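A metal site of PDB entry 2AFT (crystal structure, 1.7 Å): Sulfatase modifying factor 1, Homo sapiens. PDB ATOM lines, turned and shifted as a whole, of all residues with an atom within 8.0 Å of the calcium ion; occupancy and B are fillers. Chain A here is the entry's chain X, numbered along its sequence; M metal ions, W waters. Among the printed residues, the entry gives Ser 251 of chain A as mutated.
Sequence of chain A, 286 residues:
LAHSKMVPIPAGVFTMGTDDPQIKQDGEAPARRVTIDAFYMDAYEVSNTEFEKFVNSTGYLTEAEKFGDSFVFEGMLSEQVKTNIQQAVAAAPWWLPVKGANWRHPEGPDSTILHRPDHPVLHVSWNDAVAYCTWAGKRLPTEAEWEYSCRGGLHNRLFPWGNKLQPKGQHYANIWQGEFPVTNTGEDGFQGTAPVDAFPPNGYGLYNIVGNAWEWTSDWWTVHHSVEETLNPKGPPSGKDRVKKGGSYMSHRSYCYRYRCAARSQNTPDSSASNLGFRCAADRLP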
ATOM      1  N   HIS A 171      16.750 -13.054 -17.080  1.00  0.00           N
ATOM      2  CA  HIS A 171      17.303 -13.425 -15.798  1.00  0.00           C
ATOM      3  C   HIS A 171      16.781 -12.486 -14.706  1.00  0.00           C
ATOM      4  O   HIS A 171      16.847 -11.253 -14.855  1.00  0.00           O
ATOM      5  CB  HIS A 171      18.846 -13.416 -15.834  1.00  0.00           C
ATOM      6  CG  HIS A 171      19.412 -14.622 -16.515  1.00  0.00           C
ATOM      7  ND1 HIS A 171      19.411 -15.861 -15.914  1.00  0.00           N
ATOM      8  CD2 HIS A 171      19.818 -14.813 -17.790  1.00  0.00           C
ATOM      9  CE1 HIS A 171      19.871 -16.755 -16.777  1.00  0.00           C
ATOM     10  NE2 HIS A 171      20.132 -16.147 -17.921  1.00  0.00           N
ATOM     11  N   ALA A 173      17.694 -13.087 -11.194  1.00  0.00           N
ATOM     12  CA  ALA A 173      18.549 -13.185 -10.019  1.00  0.00           C
ATOM     13  C   ALA A 173      19.899 -13.693 -10.450  1.00  0.00           C
ATOM     14  O   ALA A 173      20.043 -14.330 -11.522  1.00  0.00           O
ATOM     15  CB  ALA A 173      17.958 -14.112  -9.037  1.00  0.00           C
ATOM     16  N   ASN A 174      20.880 -13.393  -9.620  1.00  0.00           N
ATOM     17  CA  ASN A 174      22.248 -13.788  -9.868  1.00  0.00           C
ATOM     18  C   ASN A 174      22.549 -15.121  -9.174  1.00  0.00           C
ATOM     19  O   ASN A 174      22.808 -15.164  -7.997  1.00  0.00           O
ATOM     20  CB  ASN A 174      23.200 -12.699  -9.387  1.00  0.00           C
ATOM     21  CG  ASN A 174      24.651 -13.063  -9.578  1.00  0.00           C
ATOM     22  OD1 ASN A 174      24.947 -13.920 -10.439  1.00  0.00           O
ATOM     23  ND2 ASN A 174      25.561 -12.446  -8.799  1.00  0.00           N
ATOM     24  N   ILE A 175      22.485 -16.204  -9.941  1.00  0.00           N
ATOM     25  CA  ILE A 175      22.844 -17.542  -9.487  1.00  0.00           C
ATOM     26  C   ILE A 175      23.902 -18.138 -10.445  1.00  0.00           C
ATOM     27  O   ILE A 175      24.511 -17.411 -11.210  1.00  0.00           O
ATOM     28  CB  ILE A 175      21.586 -18.417  -9.313  1.00  0.00           C
ATOM     29  CG1 ILE A 175      20.815 -18.582 -10.632  1.00  0.00           C
ATOM     30  CG2 ILE A 175      20.715 -17.810  -8.201  1.00  0.00           C
ATOM     31  CD1 ILE A 175      19.709 -19.634 -10.604  1.00  0.00           C
ATOM     32  N   TRP A 176      24.070 -19.451 -10.440  1.00  0.00           N
ATOM     33  CA  TRP A 176      25.063 -20.086 -11.301  1.00  0.00           C
ATOM     34  C   TRP A 176      24.410 -20.571 -12.589  1.00  0.00           C
ATOM     35  O   TRP A 176      23.289 -21.098 -12.555  1.00  0.00           O
ATOM     36  CB  TRP A 176      25.612 -21.287 -10.564  1.00  0.00           C
ATOM     37  CG  TRP A 176      26.741 -22.018 -11.202  1.00  0.00           C
ATOM     38  CD1 TRP A 176      26.696 -22.904 -12.235  1.00  0.00           C
ATOM     39  CD2 TRP A 176      28.098 -21.928 -10.796  1.00  0.00           C
ATOM     40  NE1 TRP A 176      27.961 -23.385 -12.490  1.00  0.00           N
ATOM     41  CE2 TRP A 176      28.839 -22.803 -11.617  1.00  0.00           C
ATOM     42  CE3 TRP A 176      28.774 -21.169  -9.825  1.00  0.00           C
ATOM     43  CZ2 TRP A 176      30.226 -22.941 -11.479  1.00  0.00           C
ATOM     44  CZ3 TRP A 176      30.152 -21.321  -9.668  1.00  0.00           C
ATOM     45  CH2 TRP A 176      30.863 -22.209 -10.505  1.00  0.00           C
ATOM     46  N   GLN A 177      25.120 -20.411 -13.712  1.00  0.00           N
ATOM     47  CA  GLN A 177      24.759 -21.123 -14.916  1.00  0.00           C
ATOM     48  C   GLN A 177      25.955 -21.927 -15.331  1.00  0.00           C
ATOM     49  O   GLN A 177      27.092 -21.444 -15.221  1.00  0.00           O
ATOM     50  CB  GLN A 177      24.384 -20.180 -16.053  1.00  0.00           C
ATOM     51  CG  GLN A 177      23.073 -19.459 -15.811  1.00  0.00           C
ATOM     52  CD  GLN A 177      23.314 -18.175 -15.074  1.00  0.00           C
ATOM     53  OE1 GLN A 177      24.283 -17.455 -15.389  1.00  0.00           O
ATOM     54  NE2 GLN A 177      22.440 -17.863 -14.079  1.00  0.00           N
ATOM     55  N   ASN A 184      31.250 -21.754 -14.511  1.00  0.00           N
ATOM     56  CA  ASN A 184      30.193 -20.753 -14.426  1.00  0.00           C
ATOM     57  C   ASN A 184      30.240 -19.917 -15.678  1.00  0.00           C
ATOM     58  O   ASN A 184      31.197 -19.167 -15.895  1.00  0.00           O
ATOM     59  CB  ASN A 184      30.403 -19.835 -13.224  1.00  0.00           C
ATOM     60  CG  ASN A 184      29.203 -18.954 -12.947  1.00  0.00           C
ATOM     61  OD1 ASN A 184      28.326 -18.789 -13.793  1.00  0.00           O
ATOM     62  ND2 ASN A 184      29.149 -18.422 -11.720  1.00  0.00           N
ATOM     63  N   THR A 185      29.238 -20.063 -16.537  1.00  0.00           N
ATOM     64  CA  THR A 185      29.232 -19.365 -17.800  1.00  0.00           C
ATOM     65  C   THR A 185      29.039 -17.851 -17.689  1.00  0.00           C
ATOM     66  O   THR A 185      29.364 -17.124 -18.616  1.00  0.00           O
ATOM     67  CB  THR A 185      28.141 -19.929 -18.735  1.00  0.00           C
ATOM     68  OG1 THR A 185      26.880 -19.603 -18.181  1.00  0.00           O
ATOM     69  CG2 THR A 185      28.238 -21.415 -18.893  1.00  0.00           C
ATOM     70  N   GLY A 186      28.486 -17.365 -16.573  1.00  0.00           N
ATOM     71  CA  GLY A 186      28.239 -15.936 -16.422  1.00  0.00           C
ATOM     72  C   GLY A 186      27.142 -15.462 -17.365  1.00  0.00           C
ATOM     73  O   GLY A 186      27.075 -14.273 -17.704  1.00  0.00           O
ATOM     74  N   GLU A 187      26.260 -16.374 -17.753  1.00  0.00           N
ATOM     75  CA  GLU A 187      25.136 -16.041 -18.627  1.00  0.00           C
ATOM     76  C   GLU A 187      24.300 -14.892 -18.083  1.00  0.00           C
ATOM     77  O   GLU A 187      23.853 -14.024 -18.856  1.00  0.00           O
ATOM     78  CB  GLU A 187      24.262 -17.264 -18.836  1.00  0.00           C
ATOM     79  CG  GLU A 187      23.090 -17.074 -19.733  1.00  0.00           C
ATOM     80  CD  GLU A 187      22.127 -18.277 -19.705  1.00  0.00           C
ATOM     81  OE1 GLU A 187      22.605 -19.419 -19.481  1.00  0.00           O
ATOM     82  OE2 GLU A 187      20.930 -18.042 -19.912  1.00  0.00           O
ATOM     83  N   ASP A 188      24.095 -14.855 -16.764  1.00  0.00           N
ATOM     84  CA  ASP A 188      23.225 -13.844 -16.172  1.00  0.00           C
ATOM     85  C   ASP A 188      23.893 -12.481 -16.010  1.00  0.00           C
ATOM     86  O   ASP A 188      23.240 -11.520 -15.575  1.00  0.00           O
ATOM     87  CB  ASP A 188      22.598 -14.315 -14.869  1.00  0.00           C
ATOM     88  CG  ASP A 188      23.598 -14.586 -13.802  1.00  0.00           C
ATOM     89  OD1 ASP A 188      24.731 -14.036 -13.883  1.00  0.00           O
ATOM     90  OD2 ASP A 188      23.253 -15.342 -12.846  1.00  0.00           O
ATOM     91  N   GLY A 189      25.176 -12.395 -16.390  1.00  0.00           N
ATOM     92  CA  GLY A 189      25.884 -11.131 -16.384  1.00  0.00           C
ATOM     93  C   GLY A 189      26.909 -10.992 -15.258  1.00  0.00           C
ATOM     94  O   GLY A 189      27.691 -10.033 -15.230  1.00  0.00           O
ATOM     95  N   PHE A 190      26.938 -11.978 -14.333  1.00  0.00           N
ATOM     96  CA  PHE A 190      27.820 -11.941 -13.191  1.00  0.00           C
ATOM     97  C   PHE A 190      28.321 -13.308 -12.811  1.00  0.00           C
ATOM     98  O   PHE A 190      27.533 -14.191 -12.566  1.00  0.00           O
ATOM     99  CB  PHE A 190      27.086 -11.310 -12.020  1.00  0.00           C
ATOM    100  CG  PHE A 190      26.562  -9.940 -12.344  1.00  0.00           C
ATOM    101  CD1 PHE A 190      27.390  -8.837 -12.235  1.00  0.00           C
ATOM    102  CD2 PHE A 190      25.261  -9.766 -12.804  1.00  0.00           C
ATOM    103  CE1 PHE A 190      26.925  -7.555 -12.568  1.00  0.00           C
ATOM    104  CE2 PHE A 190      24.799  -8.491 -13.125  1.00  0.00           C
ATOM    105  CZ  PHE A 190      25.653  -7.387 -13.004  1.00  0.00           C
ATOM    106  N   GLN A 191      29.620 -13.499 -12.756  1.00  0.00           N
ATOM    107  CA  GLN A 191      30.191 -14.737 -12.244  1.00  0.00           C
ATOM    108  C   GLN A 191      30.195 -14.756 -10.714  1.00  0.00           C
ATOM    109  O   GLN A 191      29.755 -15.716 -10.094  1.00  0.00           O
ATOM    110  CB  GLN A 191      31.571 -14.935 -12.812  1.00  0.00           C
ATOM    111  CG  GLN A 191      31.393 -15.366 -14.256  1.00  0.00           C
ATOM    112  CD  GLN A 191      32.655 -15.537 -14.965  1.00  0.00           C
ATOM    113  OE1 GLN A 191      33.540 -14.669 -14.882  1.00  0.00           O
ATOM    114  NE2 GLN A 191      32.755 -16.615 -15.770  1.00  0.00           N
ATOM    115  N   GLY A 192      30.737 -13.703 -10.122  1.00  0.00           N
ATOM    116  CA  GLY A 192      30.650 -13.515  -8.677  1.00  0.00           C
ATOM    117  C   GLY A 192      29.420 -12.694  -8.344  1.00  0.00           C
ATOM    118  O   GLY A 192      28.372 -12.860  -8.939  1.00  0.00           O
ATOM    119  N   THR A 193      29.569 -11.793  -7.372  1.00  0.00           N
ATOM    120  CA  THR A 193      28.467 -10.978  -6.979  1.00  0.00           C
ATOM    121  C   THR A 193      28.161  -9.944  -8.051  1.00  0.00           C
ATOM    122  O   THR A 193      28.964  -9.681  -8.987  1.00  0.00           O
ATOM    123  CB  THR A 193      28.763 -10.218  -5.649  1.00  0.00           C
ATOM    124  OG1 THR A 193      29.975  -9.482  -5.779  1.00  0.00           O
ATOM    125  CG2 THR A 193      28.907 -11.195  -4.491  1.00  0.00           C
ATOM    126  N   ALA A 194      26.957  -9.402  -7.922  1.00  0.00           N
ATOM    127  CA  ALA A 194      26.496  -8.272  -8.696  1.00  0.00           C
ATOM    128  C   ALA A 194      26.231  -7.077  -7.766  1.00  0.00           C
ATOM    129  O   ALA A 194      26.008  -7.260  -6.573  1.00  0.00           O
ATOM    130  CB  ALA A 194      25.184  -8.634  -9.419  1.00  0.00           C
ATOM    131  N   PHE A 199      19.247  -6.471 -11.159  1.00  0.00           N
ATOM    132  CA  PHE A 199      18.083  -7.326 -11.398  1.00  0.00           C
ATOM    133  C   PHE A 199      16.770  -6.659 -10.990  1.00  0.00           C
ATOM    134  O   PHE A 199      16.790  -5.642 -10.296  1.00  0.00           O
ATOM    135  CB  PHE A 199      18.295  -8.723 -10.815  1.00  0.00           C
ATOM    136  CG  PHE A 199      19.436  -9.455 -11.481  1.00  0.00           C
ATOM    137  CD1 PHE A 199      19.284 -10.015 -12.745  1.00  0.00           C
ATOM    138  CD2 PHE A 199      20.663  -9.484 -10.877  1.00  0.00           C
ATOM    139  CE1 PHE A 199      20.344 -10.654 -13.372  1.00  0.00           C
ATOM    140  CE2 PHE A 199      21.731 -10.136 -11.502  1.00  0.00           C
ATOM    141  CZ  PHE A 199      21.581 -10.685 -12.737  1.00  0.00           C
ATOM    142  N   ASN A 212      22.689 -13.832  -5.445  1.00  0.00           N
ATOM    143  CA  ASN A 212      23.724 -12.846  -5.114  1.00  0.00           C
ATOM    144  C   ASN A 212      24.454 -13.252  -3.829  1.00  0.00           C
ATOM    145  O   ASN A 212      25.287 -14.147  -3.920  1.00  0.00           O
ATOM    146  CB  ASN A 212      23.191 -11.384  -5.123  1.00  0.00           C
ATOM    147  CG  ASN A 212      24.243 -10.372  -5.661  1.00  0.00           C
ATOM    148  OD1 ASN A 212      25.026 -10.722  -6.536  1.00  0.00           O
ATOM    149  ND2 ASN A 212      24.234  -9.128  -5.144  1.00  0.00           N
ATOM    150  N   SER A 248      22.656 -17.871  -3.342  1.00  0.00           N
ATOM    151  CA  SER A 248      23.710 -16.987  -3.737  1.00  0.00           C
ATOM    152  C   SER A 248      24.054 -17.144  -5.224  1.00  0.00           C
ATOM    153  O   SER A 248      23.486 -17.980  -5.910  1.00  0.00           O
ATOM    154  CB  SER A 248      24.957 -17.283  -2.918  1.00  0.00           C
ATOM    155  OG  SER A 248      25.589 -18.479  -3.381  1.00  0.00           O
ATOM    156  N   TYR A 249      25.041 -16.374  -5.655  1.00  0.00           N
ATOM    157  CA  TYR A 249      25.605 -16.490  -7.012  1.00  0.00           C
ATOM    158  C   TYR A 249      26.184 -17.860  -7.360  1.00  0.00           C
ATOM    159  O   TYR A 249      26.419 -18.161  -8.536  1.00  0.00           O
ATOM    160  CB  TYR A 249      26.664 -15.410  -7.234  1.00  0.00           C
ATOM    161  CG  TYR A 249      27.959 -15.555  -6.429  1.00  0.00           C
ATOM    162  CD1 TYR A 249      28.199 -14.789  -5.270  1.00  0.00           C
ATOM    163  CD2 TYR A 249      28.951 -16.394  -6.869  1.00  0.00           C
ATOM    164  CE1 TYR A 249      29.423 -14.910  -4.566  1.00  0.00           C
ATOM    165  CE2 TYR A 249      30.178 -16.514  -6.190  1.00  0.00           C
ATOM    166  CZ  TYR A 249      30.406 -15.781  -5.038  1.00  0.00           C
ATOM    167  OH  TYR A 249      31.641 -15.923  -4.412  1.00  0.00           O
ATOM    168  N   MET A 250      26.338 -18.708  -6.341  1.00  0.00           N
ATOM    169  CA  MET A 250      26.808 -20.101  -6.509  1.00  0.00           C
ATOM    170  C   MET A 250      25.686 -21.111  -6.658  1.00  0.00           C
ATOM    171  O   MET A 250      25.930 -22.286  -6.993  1.00  0.00           O
ATOM    172  CB  MET A 250      27.655 -20.526  -5.314  1.00  0.00           C
ATOM    173  CG  MET A 250      29.021 -19.886  -5.298  1.00  0.00           C
ATOM    174  SD  MET A 250      29.892 -20.127  -3.707  1.00  0.00           S
ATOM    175  CE  MET A 250      30.144 -21.906  -3.779  1.00  0.00           C
ATOM    176  N   SER A 251      24.446 -20.697  -6.369  1.00  0.00           N
ATOM    177  CA  SER A 251      23.368 -21.654  -6.338  1.00  0.00           C
ATOM    178  C   SER A 251      22.995 -22.194  -7.718  1.00  0.00           C
ATOM    179  O   SER A 251      23.049 -21.478  -8.693  1.00  0.00           O
ATOM    180  CB  SER A 251      22.135 -21.051  -5.705  1.00  0.00           C
ATOM    181  OG  SER A 251      22.381 -20.647  -4.361  1.00  0.00           O
HETATM  182 CA    CA M   1      25.593 -15.449 -11.994  1.00  0.00          CA
HETATM  183  O   HOH W   1      26.381 -16.869 -13.829  1.00  0.00           O
HETATM  184  O   HOH W   2      27.167 -16.484 -10.505  1.00  0.00           O
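The backbone carbonyl oxygen of Asn 174 sits close to the backbone NH of Tyr 249 (3.5 Å).
The side-chain amide nitrogen (ND2) of Asn 174 is in hydrogen-bond range of the backbone carbonyl oxygen (O) of Gly 192, at 2.8 Å.
The backbone carbonyl oxygen (O) of Asn 174 sits at hydrogen-bond distance from the backbone NH (N) of Asn 212 (2.9 Å).
The side-chain amide nitrogen of Asn 174 sits close to the backbone NH of Ala 194, 3.5 Å away.
N of Asp 188 lies within hydrogen-bond range of OE1 of Gln 177 (2.9 Å).
Of the 23 residues printed, 4 come within 4 Å of the calcium ion.
The calcium ion is bound by the side-chain amide oxygen (OD1) of Asn 174 (2.3 Å), the backbone carbonyl oxygen (O) of Ile 175 (2.4 Å), the backbone carbonyl oxygen (O) of Phe 190 (2.4 Å), water W2 (2.4 Å), water W1 (2.5 Å), the side-chain carboxylate (OD2) of Asp 188 (2.5 Å) and the side-chain carboxylate (OD1) of Asp 188 (2.5 Å).
Water W1 lies within hydrogen-bond range of the side-chain amide oxygen of Gln 177 (2.7 Å), the side-chain amide oxygen of Asn 184 (2.7 Å) and the backbone NH of Gly 186 (3.5 Å).
Water W2 lies within hydrogen-bond range of O of Tyr 249 (2.7 Å), O of Gln 191 (2.7 Å) and ND2 of Asn 184 (3.0 Å).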
